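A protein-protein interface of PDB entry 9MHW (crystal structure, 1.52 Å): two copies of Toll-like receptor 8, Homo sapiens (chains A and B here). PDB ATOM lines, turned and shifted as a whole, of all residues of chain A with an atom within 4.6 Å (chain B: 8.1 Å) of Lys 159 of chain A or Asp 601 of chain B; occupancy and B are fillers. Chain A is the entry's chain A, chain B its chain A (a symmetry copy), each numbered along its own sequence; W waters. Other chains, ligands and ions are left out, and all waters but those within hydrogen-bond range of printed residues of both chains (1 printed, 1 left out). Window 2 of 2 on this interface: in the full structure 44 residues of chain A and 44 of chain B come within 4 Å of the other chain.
No position is printed for both chains.
O of Asn 130 of chain A lies within hydrogen-bond range of NZ of Lys 159 of chain A (2.9 Å). The side-chain amino group (NZ) of Lys 159 of chain A sits at hydrogen-bond distance from the side-chain amide oxygen (OD1) of Asn 131 of chain A, 3.0 Å away. The backbone NH of Tyr 156 of chain A sits at hydrogen-bond distance from the side-chain sulfur of Cys 161 of chain A, 3.8 Å away. The backbone NH (N) of Asp 601 of chain B is in hydrogen-bond range of the side-chain amide oxygen (OD1) of Asn 599 of chain B (2.9 Å). OD2 of Asp 602 of chain B is in salt-bridge range of NH2 of Arg 604 of chain B, at 2.8 Å. SG of Cys 161 of chain A is disulfide-bonded to SG of Cys 155 of chain A (2.0 Å).
Water W1 bridges the side-chain carboxylate of Asp 601 of chain B and the side-chain hydroxyl of Tyr 156 of chain A.
Of the 12 printed residues of chain B, 4 touch a printed residue of chain A. Of the 12 printed residues of chain A, 5 touch a printed residue of chain B. Hydrophobic or aromatic side chains of chain A that line the printed part of chain B: Tyr 156, Phe 157 and Pro 240. Along chain A the printed residues that touch a printed residue of chain B span positions 156 to 240. Among the printed residues, 9 pairs touch across the chains. Among the printed residues, no Asp or Glu carboxylate lies within 4 Å of a Lys or Arg side-chain nitrogen of the other chain.
O of Asp 601 of chain B touches CB of Phe 157 of chain A, at 3.3 Å. Asp 602 of chain B touches Asn 158 of chain A. CB of Lys 159 of chain A touches OD1 of Asp 601 of chain B, at 3.6 Å. Pro 240 of chain A touches Asp 601 of chain B (CG to O, 3.6 Å). Pro 240 of chain A touches Asp 602 of chain B. N of Pro 240 of chain A touches NH2 of Arg 604 of chain B (3.9 Å).
The side-chain carboxylate of Asp 601 of chain B sits at hydrogen-bond distance from the side-chain hydroxyl of Tyr 156 of chain A (2.8 Å). The backbone NH (N) of Asn 158 of chain A is in hydrogen-bond range of the backbone carbonyl oxygen (O) of Asp 601 of chain B, at 2.8 Å. The side-chain amide oxygen of Asn 158 of chain A is in hydrogen-bond range of the backbone NH of Asn 603 of chain B, at 3.0 Å.
Lys 159 of chain A touches just one residue of chain B: Asp 601 (3.6 Å). Of the printed residues of chain A, Asn 603 of chain B touches Asn 158. Of the printed residues of chain B, Asn 158 of chain A touches Asp 601, Asp 602 and Asn 603. Of the printed residues of chain B, Pro 240 of chain A touches Asp 601, Asp 602 and Arg 604. Printed residues of chain B within 4 Å of Phe 157 of chain A: Asp 601. Of the printed residues of chain A, Arg 604 of chain B touches Pro 240. Cys 161 of chain A touches none of the printed residues of chain B. The nearest residue of chain B that does not touch Lys 159 of chain A is Asp 600 of chain B (5.1 Å). The nearest printed residue of chain A that does not touch Asp 601 of chain B is Val 160 of chain A (6.0 Å). The nearest printed residue of chain B that does not touch Asn 158 of chain A is Arg 604 of chain B (4.5 Å).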
ATOM      1  N   ASN A 130      38.580  -3.071  25.533  1.00  0.00           N
ATOM      2  CA  ASN A 130      39.009  -3.381  24.174  1.00  0.00           C
ATOM      3  C   ASN A 130      39.204  -4.912  24.086  1.00  0.00           C
ATOM      4  O   ASN A 130      38.677  -5.626  24.940  1.00  0.00           O
ATOM      5  CB  ASN A 130      40.271  -2.574  23.828  1.00  0.00           C
ATOM      6  CG  ASN A 130      39.946  -1.147  23.486  1.00  0.00           C
ATOM      7  OD1 ASN A 130      39.261  -0.867  22.498  1.00  0.00           O
ATOM      8  ND2 ASN A 130      40.402  -0.229  24.295  1.00  0.00           N
ATOM      9  N   ASN A 131      39.818  -5.422  23.004  1.00  0.00           N
ATOM     10  CA  ASN A 131      40.075  -6.848  22.791  1.00  0.00           C
ATOM     11  C   ASN A 131      41.589  -7.094  22.810  1.00  0.00           C
ATOM     12  O   ASN A 131      42.109  -7.854  21.992  1.00  0.00           O
ATOM     13  CB  ASN A 131      39.489  -7.263  21.434  1.00  0.00           C
ATOM     14  CG  ASN A 131      38.009  -7.012  21.327  1.00  0.00           C
ATOM     15  OD1 ASN A 131      37.282  -6.975  22.325  1.00  0.00           O
ATOM     16  ND2 ASN A 131      37.519  -6.862  20.106  1.00  0.00           N
ATOM     17  N   TYR A 133      44.705  -8.708  24.323  1.00  0.00           N
ATOM     18  CA  TYR A 133      45.086  -9.855  25.149  1.00  0.00           C
ATOM     19  C   TYR A 133      46.605 -10.069  25.198  1.00  0.00           C
ATOM     20  O   TYR A 133      47.035 -11.097  25.704  1.00  0.00           O
ATOM     21  CB  TYR A 133      44.408 -11.130  24.628  1.00  0.00           C
ATOM     22  CG  TYR A 133      42.947 -10.919  24.269  1.00  0.00           C
ATOM     23  CD1 TYR A 133      42.069 -10.340  25.172  1.00  0.00           C
ATOM     24  CD2 TYR A 133      42.472 -11.215  23.000  1.00  0.00           C
ATOM     25  CE1 TYR A 133      40.763 -10.046  24.816  1.00  0.00           C
ATOM     26  CE2 TYR A 133      41.141 -11.018  22.665  1.00  0.00           C
ATOM     27  CZ  TYR A 133      40.291 -10.405  23.568  1.00  0.00           C
ATOM     28  OH  TYR A 133      38.974 -10.163  23.257  1.00  0.00           O
ATOM     29  N   ASN A 154      39.407  -6.153  29.408  1.00  0.00           N
ATOM     30  CA  ASN A 154      39.611  -6.660  28.044  1.00  0.00           C
ATOM     31  C   ASN A 154      39.186  -8.133  27.952  1.00  0.00           C
ATOM     32  O   ASN A 154      38.795  -8.563  26.871  1.00  0.00           O
ATOM     33  CB  ASN A 154      41.033  -6.428  27.538  1.00  0.00           C
ATOM     34  CG  ASN A 154      41.267  -5.000  27.072  1.00  0.00           C
ATOM     35  OD1 ASN A 154      41.444  -4.747  25.890  1.00  0.00           O
ATOM     36  ND2 ASN A 154      41.178  -4.029  27.966  1.00  0.00           N
ATOM     37  N   CYS A 155      39.238  -8.903  29.055  1.00  0.00           N
ATOM     38  CA  CYS A 155      38.796 -10.296  29.010  1.00  0.00           C
ATOM     39  C   CYS A 155      38.169 -10.692  30.323  1.00  0.00           C
ATOM     40  O   CYS A 155      38.867 -10.827  31.326  1.00  0.00           O
ATOM     41  CB  CYS A 155      39.942 -11.220  28.628  1.00  0.00           C
ATOM     42  SG  CYS A 155      39.463 -12.965  28.534  1.00  0.00           S
ATOM     43  N   TYR A 156      36.857 -10.908  30.323  1.00  0.00           N
ATOM     44  CA  TYR A 156      36.130 -11.139  31.555  1.00  0.00           C
ATOM     45  C   TYR A 156      34.792 -11.809  31.323  1.00  0.00           C
ATOM     46  O   TYR A 156      34.293 -11.842  30.200  1.00  0.00           O
ATOM     47  CB  TYR A 156      35.878  -9.779  32.233  1.00  0.00           C
ATOM     48  CG  TYR A 156      35.137  -8.815  31.330  1.00  0.00           C
ATOM     49  CD1 TYR A 156      35.814  -8.058  30.385  1.00  0.00           C
ATOM     50  CD2 TYR A 156      33.753  -8.752  31.336  1.00  0.00           C
ATOM     51  CE1 TYR A 156      35.134  -7.267  29.468  1.00  0.00           C
ATOM     52  CE2 TYR A 156      33.065  -7.928  30.459  1.00  0.00           C
ATOM     53  CZ  TYR A 156      33.758  -7.183  29.524  1.00  0.00           C
ATOM     54  OH  TYR A 156      33.061  -6.366  28.659  1.00  0.00           O
ATOM     55  N   PHE A 157      34.195 -12.342  32.406  1.00  0.00           N
ATOM     56  CA  PHE A 157      32.873 -12.975  32.396  1.00  0.00           C
ATOM     57  C   PHE A 157      32.802 -14.034  31.259  1.00  0.00           C
ATOM     58  O   PHE A 157      33.790 -14.742  31.076  1.00  0.00           O
ATOM     59  CB  PHE A 157      31.789 -11.866  32.308  1.00  0.00           C
ATOM     60  CG  PHE A 157      31.738 -10.834  33.408  1.00  0.00           C
ATOM     61  CD1 PHE A 157      32.397 -11.038  34.611  1.00  0.00           C
ATOM     62  CD2 PHE A 157      30.948  -9.706  33.279  1.00  0.00           C
ATOM     63  CE1 PHE A 157      32.344 -10.081  35.617  1.00  0.00           C
ATOM     64  CE2 PHE A 157      30.904  -8.753  34.288  1.00  0.00           C
ATOM     65  CZ  PHE A 157      31.574  -8.967  35.459  1.00  0.00           C
ATOM     66  N   ASN A 158      31.716 -14.110  30.466  1.00  0.00           N
ATOM     67  CA  ASN A 158      31.625 -15.051  29.363  1.00  0.00           C
ATOM     68  C   ASN A 158      31.963 -14.421  28.018  1.00  0.00           C
ATOM     69  O   ASN A 158      31.528 -14.936  26.992  1.00  0.00           O
ATOM     70  CB  ASN A 158      30.231 -15.664  29.330  1.00  0.00           C
ATOM     71  CG  ASN A 158      29.811 -16.285  30.630  1.00  0.00           C
ATOM     72  OD1 ASN A 158      28.657 -16.143  31.051  1.00  0.00           O
ATOM     73  ND2 ASN A 158      30.695 -17.048  31.282  1.00  0.00           N
ATOM     74  N   LYS A 159      32.781 -13.354  27.997  1.00  0.00           N
ATOM     75  CA  LYS A 159      33.232 -12.773  26.739  1.00  0.00           C
ATOM     76  C   LYS A 159      34.174 -13.781  26.079  1.00  0.00           C
ATOM     77  O   LYS A 159      34.971 -14.412  26.772  1.00  0.00           O
ATOM     78  CB  LYS A 159      34.009 -11.468  26.985  1.00  0.00           C
ATOM     79  CG  LYS A 159      34.592 -10.842  25.724  1.00  0.00           C
ATOM     80  CD  LYS A 159      35.500  -9.675  26.065  1.00  0.00           C
ATOM     81  CE  LYS A 159      36.102  -9.080  24.829  1.00  0.00           C
ATOM     82  NZ  LYS A 159      36.801  -7.809  25.131  1.00  0.00           N
ATOM     83  N   VAL A 160      34.064 -13.945  24.754  1.00  0.00           N
ATOM     84  CA  VAL A 160      34.963 -14.825  24.008  1.00  0.00           C
ATOM     85  C   VAL A 160      36.263 -14.053  23.915  1.00  0.00           C
ATOM     86  O   VAL A 160      36.302 -13.022  23.247  1.00  0.00           O
ATOM     87  CB  VAL A 160      34.401 -15.164  22.601  1.00  0.00           C
ATOM     88  CG1 VAL A 160      35.488 -15.750  21.691  1.00  0.00           C
ATOM     89  CG2 VAL A 160      33.206 -16.113  22.713  1.00  0.00           C
ATOM     90  N   CYS A 161      37.285 -14.483  24.652  1.00  0.00           N
ATOM     91  CA  CYS A 161      38.552 -13.764  24.684  1.00  0.00           C
ATOM     92  C   CYS A 161      39.691 -14.696  25.095  1.00  0.00           C
ATOM     93  O   CYS A 161      39.451 -15.785  25.617  1.00  0.00           O
ATOM     94  CB  CYS A 161      38.449 -12.553  25.616  1.00  0.00           C
ATOM     95  SG  CYS A 161      37.842 -12.927  27.282  1.00  0.00           S
ATOM     96  N   PRO A 240      28.466 -13.376  35.606  1.00  0.00           N
ATOM     97  CA  PRO A 240      29.005 -14.747  35.545  1.00  0.00           C
ATOM     98  C   PRO A 240      30.189 -14.837  36.506  1.00  0.00           C
ATOM     99  O   PRO A 240      31.055 -13.963  36.487  1.00  0.00           O
ATOM    100  CB  PRO A 240      29.416 -14.908  34.074  1.00  0.00           C
ATOM    101  CG  PRO A 240      28.609 -13.884  33.356  1.00  0.00           C
ATOM    102  CD  PRO A 240      28.606 -12.711  34.300  1.00  0.00           C
ATOM    103  N   ASP B 595      17.862  -6.152  28.738  1.00  0.00           N
ATOM    104  CA  ASP B 595      19.135  -5.569  28.301  1.00  0.00           C
ATOM    105  C   ASP B 595      20.280  -6.071  29.209  1.00  0.00           C
ATOM    106  O   ASP B 595      21.371  -6.356  28.709  1.00  0.00           O
ATOM    107  CB  ASP B 595      19.070  -4.036  28.303  1.00  0.00           C
ATOM    108  CG  ASP B 595      18.879  -3.401  29.676  1.00  0.00           C
ATOM    109  OD1 ASP B 595      17.989  -3.866  30.432  1.00  0.00           O
ATOM    110  OD2 ASP B 595      19.583  -2.426  29.974  1.00  0.00           O
ATOM    111  N   ILE B 596      20.008  -6.242  30.523  1.00  0.00           N
ATOM    112  CA  ILE B 596      20.978  -6.768  31.473  1.00  0.00           C
ATOM    113  C   ILE B 596      21.015  -8.303  31.380  1.00  0.00           C
ATOM    114  O   ILE B 596      22.088  -8.860  31.256  1.00  0.00           O
ATOM    115  CB  ILE B 596      20.653  -6.306  32.917  1.00  0.00           C
ATOM    116  CG1 ILE B 596      20.702  -4.745  33.033  1.00  0.00           C
ATOM    117  CG2 ILE B 596      21.581  -6.998  33.924  1.00  0.00           C
ATOM    118  CD1 ILE B 596      20.440  -4.154  34.439  1.00  0.00           C
ATOM    119  N   LEU B 597      19.854  -8.986  31.449  1.00  0.00           N
ATOM    120  CA  LEU B 597      19.816 -10.458  31.394  1.00  0.00           C
ATOM    121  C   LEU B 597      20.490 -11.011  30.140  1.00  0.00           C
ATOM    122  O   LEU B 597      21.196 -12.018  30.221  1.00  0.00           O
ATOM    123  CB  LEU B 597      18.363 -10.994  31.471  1.00  0.00           C
ATOM    124  CG  LEU B 597      17.568 -10.599  32.723  1.00  0.00           C
ATOM    125  CD1 LEU B 597      16.069 -10.546  32.469  1.00  0.00           C
ATOM    126  CD2 LEU B 597      17.865 -11.542  33.845  1.00  0.00           C
ATOM    127  N   TRP B 598      20.307 -10.331  28.996  1.00  0.00           N
ATOM    128  CA  TRP B 598      20.908 -10.755  27.744  1.00  0.00           C
ATOM    129  C   TRP B 598      22.117  -9.925  27.365  1.00  0.00           C
ATOM    130  O   TRP B 598      22.425  -9.808  26.183  1.00  0.00           O
ATOM    131  CB  TRP B 598      19.875 -10.733  26.610  1.00  0.00           C
ATOM    132  CG  TRP B 598      18.819 -11.787  26.704  1.00  0.00           C
ATOM    133  CD1 TRP B 598      18.919 -13.016  27.290  1.00  0.00           C
ATOM    134  CD2 TRP B 598      17.550 -11.757  26.045  1.00  0.00           C
ATOM    135  NE1 TRP B 598      17.762 -13.731  27.083  1.00  0.00           N
ATOM    136  CE2 TRP B 598      16.909 -12.984  26.310  1.00  0.00           C
ATOM    137  CE3 TRP B 598      16.880 -10.795  25.281  1.00  0.00           C
ATOM    138  CZ2 TRP B 598      15.629 -13.269  25.841  1.00  0.00           C
ATOM    139  CZ3 TRP B 598      15.621 -11.092  24.791  1.00  0.00           C
ATOM    140  CH2 TRP B 598      15.008 -12.316  25.076  1.00  0.00           C
ATOM    141  N   ASN B 599      22.880  -9.446  28.350  1.00  0.00           N
ATOM    142  CA  ASN B 599      24.125  -8.729  28.069  1.00  0.00           C
ATOM    143  C   ASN B 599      25.086  -9.722  27.333  1.00  0.00           C
ATOM    144  O   ASN B 599      25.101 -10.913  27.663  1.00  0.00           O
ATOM    145  CB  ASN B 599      24.721  -8.206  29.373  1.00  0.00           C
ATOM    146  CG  ASN B 599      26.120  -7.721  29.217  1.00  0.00           C
ATOM    147  OD1 ASN B 599      27.058  -8.479  29.445  1.00  0.00           O
ATOM    148  ND2 ASN B 599      26.282  -6.475  28.783  1.00  0.00           N
ATOM    149  N   ASP B 600      25.797  -9.251  26.295  1.00  0.00           N
ATOM    150  CA  ASP B 600      26.630 -10.158  25.489  1.00  0.00           C
ATOM    151  C   ASP B 600      27.765 -10.818  26.270  1.00  0.00           C
ATOM    152  O   ASP B 600      28.278 -11.828  25.796  1.00  0.00           O
ATOM    153  CB  ASP B 600      27.169  -9.532  24.189  1.00  0.00           C
ATOM    154  CG  ASP B 600      27.329  -8.037  24.182  1.00  0.00           C
ATOM    155  OD1 ASP B 600      28.180  -7.530  24.951  1.00  0.00           O
ATOM    156  OD2 ASP B 600      26.596  -7.367  23.411  1.00  0.00           O
ATOM    157  N   ASP B 601      28.119 -10.324  27.466  1.00  0.00           N
ATOM    158  CA  ASP B 601      29.176 -10.959  28.271  1.00  0.00           C
ATOM    159  C   ASP B 601      28.629 -11.999  29.278  1.00  0.00           C
ATOM    160  O   ASP B 601      29.401 -12.542  30.073  1.00  0.00           O
ATOM    161  CB  ASP B 601      29.971  -9.880  29.026  1.00  0.00           C
ATOM    162  CG  ASP B 601      30.591  -8.852  28.100  1.00  0.00           C
ATOM    163  OD1 ASP B 601      31.157  -9.255  27.062  1.00  0.00           O
ATOM    164  OD2 ASP B 601      30.533  -7.641  28.427  1.00  0.00           O
ATOM    165  N   ASP B 602      27.314 -12.297  29.232  1.00  0.00           N
ATOM    166  CA  ASP B 602      26.707 -13.197  30.191  1.00  0.00           C
ATOM    167  C   ASP B 602      25.863 -14.213  29.433  1.00  0.00           C
ATOM    168  O   ASP B 602      24.976 -13.801  28.710  1.00  0.00           O
ATOM    169  CB  ASP B 602      25.843 -12.346  31.139  1.00  0.00           C
ATOM    170  CG  ASP B 602      25.302 -13.056  32.353  1.00  0.00           C
ATOM    171  OD1 ASP B 602      25.389 -14.302  32.405  1.00  0.00           O
ATOM    172  OD2 ASP B 602      24.798 -12.364  33.261  1.00  0.00           O
ATOM    173  N   ASN B 603      26.133 -15.522  29.586  1.00  0.00           N
ATOM    174  CA  ASN B 603      25.375 -16.575  28.890  1.00  0.00           C
ATOM    175  C   ASN B 603      24.274 -17.208  29.756  1.00  0.00           C
ATOM    176  O   ASN B 603      23.546 -18.071  29.269  1.00  0.00           O
ATOM    177  CB  ASN B 603      26.335 -17.696  28.446  1.00  0.00           C
ATOM    178  CG  ASN B 603      27.303 -17.292  27.364  1.00  0.00           C
ATOM    179  OD1 ASN B 603      27.027 -16.405  26.548  1.00  0.00           O
ATOM    180  ND2 ASN B 603      28.450 -17.956  27.310  1.00  0.00           N
ATOM    181  N   ARG B 604      24.171 -16.829  31.042  1.00  0.00           N
ATOM    182  CA  ARG B 604      23.248 -17.468  31.979  1.00  0.00           C
ATOM    183  C   ARG B 604      21.767 -17.432  31.634  1.00  0.00           C
ATOM    184  O   ARG B 604      21.068 -18.400  31.938  1.00  0.00           O
ATOM    185  CB  ARG B 604      23.431 -16.905  33.404  1.00  0.00           C
ATOM    186  CG  ARG B 604      24.805 -17.301  34.023  1.00  0.00           C
ATOM    187  CD  ARG B 604      25.066 -16.647  35.366  1.00  0.00           C
ATOM    188  NE  ARG B 604      24.988 -15.194  35.244  1.00  0.00           N
ATOM    189  CZ  ARG B 604      24.717 -14.348  36.234  1.00  0.00           C
ATOM    190  NH1 ARG B 604      24.519 -14.795  37.470  1.00  0.00           N
ATOM    191  NH2 ARG B 604      24.614 -13.049  35.992  1.00  0.00           N
ATOM    192  N   HIS B 627      20.102  -4.661  21.339  1.00  0.00           N
ATOM    193  CA  HIS B 627      20.208  -5.796  20.439  1.00  0.00           C
ATOM    194  C   HIS B 627      19.853  -7.067  21.208  1.00  0.00           C
ATOM    195  O   HIS B 627      19.988  -7.110  22.431  1.00  0.00           O
ATOM    196  CB  HIS B 627      21.624  -5.892  19.870  1.00  0.00           C
ATOM    197  CG  HIS B 627      22.669  -6.129  20.912  1.00  0.00           C
ATOM    198  ND1 HIS B 627      23.044  -5.135  21.798  1.00  0.00           N
ATOM    199  CD2 HIS B 627      23.405  -7.239  21.163  1.00  0.00           C
ATOM    200  CE1 HIS B 627      23.982  -5.667  22.563  1.00  0.00           C
ATOM    201  NE2 HIS B 627      24.234  -6.933  22.215  1.00  0.00           N
ATOM    202  N   PRO B 629      20.977 -10.942  21.508  1.00  0.00           N
ATOM    203  CA  PRO B 629      21.959 -11.933  21.004  1.00  0.00           C
ATOM    204  C   PRO B 629      21.271 -12.977  20.124  1.00  0.00           C
ATOM    205  O   PRO B 629      20.178 -13.420  20.469  1.00  0.00           O
ATOM    206  CB  PRO B 629      22.493 -12.580  22.281  1.00  0.00           C
ATOM    207  CG  PRO B 629      22.285 -11.531  23.347  1.00  0.00           C
ATOM    208  CD  PRO B 629      21.000 -10.859  22.982  1.00  0.00           C
HETATM  209  O   HOH W   1      32.549  -7.445  25.646  1.00  0.00           O
